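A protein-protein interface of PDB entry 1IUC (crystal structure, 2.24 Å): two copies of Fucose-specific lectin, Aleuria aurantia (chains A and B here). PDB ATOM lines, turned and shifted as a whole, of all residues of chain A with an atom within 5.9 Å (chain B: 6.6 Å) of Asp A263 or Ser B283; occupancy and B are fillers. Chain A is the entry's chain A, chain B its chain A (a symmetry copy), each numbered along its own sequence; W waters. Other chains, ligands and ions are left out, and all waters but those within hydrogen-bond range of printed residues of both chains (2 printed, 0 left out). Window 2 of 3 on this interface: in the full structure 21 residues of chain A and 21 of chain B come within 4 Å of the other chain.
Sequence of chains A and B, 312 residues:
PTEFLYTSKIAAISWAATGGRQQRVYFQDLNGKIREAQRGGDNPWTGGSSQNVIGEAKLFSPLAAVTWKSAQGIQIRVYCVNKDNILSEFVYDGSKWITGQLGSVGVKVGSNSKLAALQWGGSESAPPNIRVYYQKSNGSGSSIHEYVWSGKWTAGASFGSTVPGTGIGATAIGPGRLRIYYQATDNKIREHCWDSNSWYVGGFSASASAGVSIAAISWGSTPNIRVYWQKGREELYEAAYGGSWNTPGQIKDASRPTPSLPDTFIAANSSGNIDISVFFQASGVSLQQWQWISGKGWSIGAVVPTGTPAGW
The side-chain hydroxyl (OG) of Ser B283 is in hydrogen-bond range of the side-chain carboxylate (OD1) of Asp A263 (2.8 Å).
O of Pro A262 sits at hydrogen-bond distance from OH of Tyr A6 (2.7 Å). O of Ser B260 is in hydrogen-bond range of NH1 of Arg B233, at 2.8 Å. The backbone NH of Leu B261 is in hydrogen-bond range of the backbone carbonyl oxygen of Gln B281 (3.0 Å). O of Ser B283 sits at hydrogen-bond distance from OG of Ser B286.
Among the printed residues, merely in contact across the chains: Pro A262 with Arg B233, Tyr A6 with Val B285 and Tyr A6 with Leu B261.
Asp A263 touches one residue of chain B. Ser B283 touches one residue of chain A. Of the printed residues of chain A, Arg B233 touches Pro A262 (3.6 Å). Of the printed residues of chain A, Leu B261 touches Tyr A6. Phe A265 touches none of the printed residues of chain B. Thr A7 touches none of the printed residues of chain B.
Of the 10 printed residues of chain A, 3 touch a printed residue of chain B. Among the printed residues, no Asp or Glu carboxylate lies within 4 Å of a Lys or Arg side-chain nitrogen of the other chain.
Positions printed for both chains: 233 and 261. Of the 4 pairs that touch across the chains among the printed residues, none has its exchanged pair printed and touching as well.
Water W2 lies within hydrogen-bond range of the side-chain carboxylate of Asp A263, the side-chain hydroxyl of Tyr A6 and the side-chain hydroxyl of Ser B283. Water W1 lies within hydrogen-bond range of OD1 of Asp A263 and OG of Ser B283.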
ATOM      1  N   TYR A   6      22.368  16.461   5.538  1.00  0.00           N
ATOM      2  CA  TYR A   6      21.281  16.917   6.396  1.00  0.00           C
ATOM      3  C   TYR A   6      21.324  18.450   6.512  1.00  0.00           C
ATOM      4  O   TYR A   6      22.352  19.040   6.855  1.00  0.00           O
ATOM      5  CB  TYR A   6      21.398  16.274   7.781  1.00  0.00           C
ATOM      6  CG  TYR A   6      20.361  16.770   8.763  1.00  0.00           C
ATOM      7  CD1 TYR A   6      19.001  16.710   8.456  1.00  0.00           C
ATOM      8  CD2 TYR A   6      20.738  17.300   9.996  1.00  0.00           C
ATOM      9  CE1 TYR A   6      18.042  17.167   9.359  1.00  0.00           C
ATOM     10  CE2 TYR A   6      19.791  17.755  10.903  1.00  0.00           C
ATOM     11  CZ  TYR A   6      18.445  17.685  10.577  1.00  0.00           C
ATOM     12  OH  TYR A   6      17.506  18.139  11.468  1.00  0.00           O
ATOM     13  N   THR A   7      20.181  19.068   6.229  1.00  0.00           N
ATOM     14  CA  THR A   7      19.969  20.518   6.216  1.00  0.00           C
ATOM     15  C   THR A   7      20.607  21.179   5.004  1.00  0.00           C
ATOM     16  O   THR A   7      20.911  22.376   5.000  1.00  0.00           O
ATOM     17  CB  THR A   7      20.411  21.246   7.509  1.00  0.00           C
ATOM     18  OG1 THR A   7      21.838  21.322   7.585  1.00  0.00           O
ATOM     19  CG2 THR A   7      19.844  20.529   8.731  1.00  0.00           C
ATOM     20  N   LYS A 231       8.417  25.035   8.060  1.00  0.00           N
ATOM     21  CA  LYS A 231       9.349  24.963   9.166  1.00  0.00           C
ATOM     22  C   LYS A 231       9.528  23.451   9.306  1.00  0.00           C
ATOM     23  O   LYS A 231       8.536  22.721   9.309  1.00  0.00           O
ATOM     24  CB  LYS A 231       8.691  25.526  10.423  1.00  0.00           C
ATOM     25  CG  LYS A 231       9.529  25.442  11.678  1.00  0.00           C
ATOM     26  CD  LYS A 231      10.571  26.518  11.679  1.00  0.00           C
ATOM     27  CE  LYS A 231      11.231  26.628  13.044  1.00  0.00           C
ATOM     28  NZ  LYS A 231      12.208  27.749  13.036  1.00  0.00           N
ATOM     29  N   GLY A 232      10.772  22.984   9.389  1.00  0.00           N
ATOM     30  CA  GLY A 232      11.022  21.556   9.508  1.00  0.00           C
ATOM     31  C   GLY A 232      10.216  20.912  10.621  1.00  0.00           C
ATOM     32  O   GLY A 232      10.125  21.457  11.720  1.00  0.00           O
ATOM     33  N   ARG A 233       9.628  19.756  10.333  1.00  0.00           N
ATOM     34  CA  ARG A 233       8.822  19.021  11.304  1.00  0.00           C
ATOM     35  C   ARG A 233       7.443  19.636  11.547  1.00  0.00           C
ATOM     36  O   ARG A 233       6.757  19.278  12.506  1.00  0.00           O
ATOM     37  CB  ARG A 233       9.565  18.878  12.638  1.00  0.00           C
ATOM     38  CG  ARG A 233      10.015  17.464  12.935  1.00  0.00           C
ATOM     39  CD  ARG A 233       8.837  16.529  13.037  1.00  0.00           C
ATOM     40  NE  ARG A 233       9.214  15.150  13.366  1.00  0.00           N
ATOM     41  CZ  ARG A 233       9.818  14.292  12.538  1.00  0.00           C
ATOM     42  NH1 ARG A 233      10.145  14.644  11.296  1.00  0.00           N
ATOM     43  NH2 ARG A 233      10.076  13.058  12.953  1.00  0.00           N
ATOM     44  N   LEU A 261      12.198  16.720   8.230  1.00  0.00           N
ATOM     45  CA  LEU A 261      13.052  16.744   9.408  1.00  0.00           C
ATOM     46  C   LEU A 261      13.169  18.175   9.877  1.00  0.00           C
ATOM     47  O   LEU A 261      12.912  19.104   9.112  1.00  0.00           O
ATOM     48  CB  LEU A 261      14.436  16.198   9.072  1.00  0.00           C
ATOM     49  CG  LEU A 261      14.467  14.694   8.796  1.00  0.00           C
ATOM     50  CD1 LEU A 261      15.837  14.281   8.331  1.00  0.00           C
ATOM     51  CD2 LEU A 261      14.084  13.956  10.072  1.00  0.00           C
ATOM     52  N   PRO A 262      13.548  18.376  11.151  1.00  0.00           N
ATOM     53  CA  PRO A 262      13.697  19.723  11.704  1.00  0.00           C
ATOM     54  C   PRO A 262      14.795  20.512  10.988  1.00  0.00           C
ATOM     55  O   PRO A 262      15.733  19.930  10.451  1.00  0.00           O
ATOM     56  CB  PRO A 262      14.078  19.464  13.165  1.00  0.00           C
ATOM     57  CG  PRO A 262      13.472  18.130  13.458  1.00  0.00           C
ATOM     58  CD  PRO A 262      13.714  17.349  12.195  1.00  0.00           C
ATOM     59  N   ASP A 263      14.668  21.835  10.981  1.00  0.00           N
ATOM     60  CA  ASP A 263      15.693  22.692  10.394  1.00  0.00           C
ATOM     61  C   ASP A 263      16.054  22.444   8.925  1.00  0.00           C
ATOM     62  O   ASP A 263      17.160  22.783   8.500  1.00  0.00           O
ATOM     63  CB  ASP A 263      16.954  22.583  11.258  1.00  0.00           C
ATOM     64  CG  ASP A 263      16.663  22.827  12.727  1.00  0.00           C
ATOM     65  OD1 ASP A 263      16.990  21.961  13.571  1.00  0.00           O
ATOM     66  OD2 ASP A 263      16.091  23.891  13.038  1.00  0.00           O
ATOM     67  N   THR A 264      15.133  21.871   8.153  1.00  0.00           N
ATOM     68  CA  THR A 264      15.381  21.603   6.742  1.00  0.00           C
ATOM     69  C   THR A 264      14.781  22.659   5.802  1.00  0.00           C
ATOM     70  O   THR A 264      14.110  23.595   6.242  1.00  0.00           O
ATOM     71  CB  THR A 264      14.846  20.213   6.345  1.00  0.00           C
ATOM     72  OG1 THR A 264      13.471  20.121   6.714  1.00  0.00           O
ATOM     73  CG2 THR A 264      15.640  19.103   7.059  1.00  0.00           C
ATOM     74  N   PHE A 265      15.021  22.503   4.502  1.00  0.00           N
ATOM     75  CA  PHE A 265      14.534  23.476   3.530  1.00  0.00           C
ATOM     76  C   PHE A 265      13.656  22.859   2.439  1.00  0.00           C
ATOM     77  O   PHE A 265      13.542  21.640   2.329  1.00  0.00           O
ATOM     78  CB  PHE A 265      15.734  24.203   2.892  1.00  0.00           C
ATOM     79  CG  PHE A 265      16.663  24.824   3.900  1.00  0.00           C
ATOM     80  CD1 PHE A 265      17.722  24.097   4.431  1.00  0.00           C
ATOM     81  CD2 PHE A 265      16.404  26.097   4.408  1.00  0.00           C
ATOM     82  CE1 PHE A 265      18.511  24.612   5.464  1.00  0.00           C
ATOM     83  CE2 PHE A 265      17.180  26.628   5.447  1.00  0.00           C
ATOM     84  CZ  PHE A 265      18.238  25.877   5.979  1.00  0.00           C
ATOM     85  N   ARG B 233      13.889  11.948  19.085  1.00  0.00           N
ATOM     86  CA  ARG B 233      12.706  12.799  19.186  1.00  0.00           C
ATOM     87  C   ARG B 233      11.695  12.324  20.230  1.00  0.00           C
ATOM     88  O   ARG B 233      10.554  12.789  20.256  1.00  0.00           O
ATOM     89  CB  ARG B 233      12.013  12.939  17.825  1.00  0.00           C
ATOM     90  CG  ARG B 233      12.139  14.320  17.217  1.00  0.00           C
ATOM     91  CD  ARG B 233      11.496  15.361  18.097  1.00  0.00           C
ATOM     92  NE  ARG B 233      11.551  16.714  17.535  1.00  0.00           N
ATOM     93  CZ  ARG B 233      12.649  17.473  17.446  1.00  0.00           C
ATOM     94  NH1 ARG B 233      13.830  17.033  17.875  1.00  0.00           N
ATOM     95  NH2 ARG B 233      12.555  18.697  16.943  1.00  0.00           N
ATOM     96  N   PRO B 259      14.524  16.714  23.195  1.00  0.00           N
ATOM     97  CA  PRO B 259      15.643  17.450  22.596  1.00  0.00           C
ATOM     98  C   PRO B 259      16.491  16.761  21.526  1.00  0.00           C
ATOM     99  O   PRO B 259      17.274  17.427  20.836  1.00  0.00           O
ATOM    100  CB  PRO B 259      16.476  17.852  23.814  1.00  0.00           C
ATOM    101  CG  PRO B 259      16.279  16.691  24.748  1.00  0.00           C
ATOM    102  CD  PRO B 259      14.790  16.410  24.618  1.00  0.00           C
ATOM    103  N   SER B 260      16.355  15.449  21.367  1.00  0.00           N
ATOM    104  CA  SER B 260      17.161  14.769  20.369  1.00  0.00           C
ATOM    105  C   SER B 260      16.498  14.762  18.992  1.00  0.00           C
ATOM    106  O   SER B 260      15.269  14.865  18.868  1.00  0.00           O
ATOM    107  CB  SER B 260      17.449  13.329  20.808  1.00  0.00           C
ATOM    108  OG  SER B 260      16.289  12.516  20.734  1.00  0.00           O
ATOM    109  N   LEU B 261      17.317  14.634  17.956  1.00  0.00           N
ATOM    110  CA  LEU B 261      16.800  14.590  16.596  1.00  0.00           C
ATOM    111  C   LEU B 261      16.344  13.178  16.310  1.00  0.00           C
ATOM    112  O   LEU B 261      16.757  12.240  16.990  1.00  0.00           O
ATOM    113  CB  LEU B 261      17.885  14.991  15.602  1.00  0.00           C
ATOM    114  CG  LEU B 261      18.267  16.472  15.655  1.00  0.00           C
ATOM    115  CD1 LEU B 261      19.440  16.736  14.750  1.00  0.00           C
ATOM    116  CD2 LEU B 261      17.062  17.302  15.235  1.00  0.00           C
ATOM    117  N   GLN B 281      22.354  13.413  20.215  1.00  0.00           N
ATOM    118  CA  GLN B 281      22.556  14.358  19.126  1.00  0.00           C
ATOM    119  C   GLN B 281      21.331  15.246  18.961  1.00  0.00           C
ATOM    120  O   GLN B 281      20.212  14.755  18.771  1.00  0.00           O
ATOM    121  CB  GLN B 281      22.834  13.599  17.829  1.00  0.00           C
ATOM    122  CG  GLN B 281      23.124  14.486  16.641  1.00  0.00           C
ATOM    123  CD  GLN B 281      23.540  13.679  15.434  1.00  0.00           C
ATOM    124  OE1 GLN B 281      22.759  12.889  14.904  1.00  0.00           O
ATOM    125  NE2 GLN B 281      24.784  13.862  14.997  1.00  0.00           N
ATOM    126  N   ALA B 282      21.557  16.556  19.019  1.00  0.00           N
ATOM    127  CA  ALA B 282      20.471  17.522  18.899  1.00  0.00           C
ATOM    128  C   ALA B 282      20.647  18.487  17.732  1.00  0.00           C
ATOM    129  O   ALA B 282      21.622  18.413  16.974  1.00  0.00           O
ATOM    130  CB  ALA B 282      20.345  18.326  20.211  1.00  0.00           C
ATOM    131  N   SER B 283      19.689  19.399  17.613  1.00  0.00           N
ATOM    132  CA  SER B 283      19.693  20.417  16.576  1.00  0.00           C
ATOM    133  C   SER B 283      21.021  21.159  16.659  1.00  0.00           C
ATOM    134  O   SER B 283      21.526  21.406  17.754  1.00  0.00           O
ATOM    135  CB  SER B 283      18.538  21.386  16.818  1.00  0.00           C
ATOM    136  OG  SER B 283      18.543  22.410  15.846  1.00  0.00           O
ATOM    137  N   GLY B 284      21.595  21.520  15.517  1.00  0.00           N
ATOM    138  CA  GLY B 284      22.880  22.206  15.554  1.00  0.00           C
ATOM    139  C   GLY B 284      23.717  22.052  14.292  1.00  0.00           C
ATOM    140  O   GLY B 284      24.028  23.054  13.653  1.00  0.00           O
ATOM    141  N   VAL B 285      24.127  20.838  13.924  1.00  0.00           N
ATOM    142  CA  VAL B 285      23.871  19.588  14.643  1.00  0.00           C
ATOM    143  C   VAL B 285      24.844  19.549  15.827  1.00  0.00           C
ATOM    144  O   VAL B 285      26.063  19.606  15.645  1.00  0.00           O
ATOM    145  CB  VAL B 285      24.150  18.393  13.715  1.00  0.00           C
ATOM    146  CG1 VAL B 285      23.959  17.086  14.460  1.00  0.00           C
ATOM    147  CG2 VAL B 285      23.220  18.467  12.491  1.00  0.00           C
ATOM    148  N   SER B 286      24.316  19.441  17.038  1.00  0.00           N
ATOM    149  CA  SER B 286      25.178  19.457  18.209  1.00  0.00           C
ATOM    150  C   SER B 286      25.256  18.160  19.003  1.00  0.00           C
ATOM    151  O   SER B 286      24.369  17.311  18.934  1.00  0.00           O
ATOM    152  CB  SER B 286      24.731  20.585  19.142  1.00  0.00           C
ATOM    153  OG  SER B 286      23.367  20.411  19.473  1.00  0.00           O
ATOM    154  N   LEU B 287      26.340  18.032  19.765  1.00  0.00           N
ATOM    155  CA  LEU B 287      26.564  16.867  20.607  1.00  0.00           C
ATOM    156  C   LEU B 287      26.282  17.337  22.027  1.00  0.00           C
ATOM    157  O   LEU B 287      27.004  18.172  22.574  1.00  0.00           O
ATOM    158  CB  LEU B 287      28.013  16.381  20.477  1.00  0.00           C
ATOM    159  CG  LEU B 287      28.450  15.189  21.346  1.00  0.00           C
ATOM    160  CD1 LEU B 287      27.407  14.094  21.316  1.00  0.00           C
ATOM    161  CD2 LEU B 287      29.791  14.662  20.842  1.00  0.00           C
ATOM    162  N   GLN B 288      25.218  16.817  22.618  1.00  0.00           N
ATOM    163  CA  GLN B 288      24.869  17.239  23.961  1.00  0.00           C
ATOM    164  C   GLN B 288      24.865  16.117  24.977  1.00  0.00           C
ATOM    165  O   GLN B 288      24.988  14.948  24.628  1.00  0.00           O
ATOM    166  CB  GLN B 288      23.523  17.957  23.922  1.00  0.00           C
ATOM    167  CG  GLN B 288      23.631  19.233  23.108  1.00  0.00           C
ATOM    168  CD  GLN B 288      22.525  20.225  23.388  1.00  0.00           C
ATOM    169  OE1 GLN B 288      22.107  20.403  24.537  1.00  0.00           O
ATOM    170  NE2 GLN B 288      22.060  20.901  22.338  1.00  0.00           N
HETATM  171  O   HOH W   1      15.120  21.893  15.737  1.00  0.00           O
HETATM  172  O   HOH W   2      18.795  20.299  13.173  1.00  0.00           O
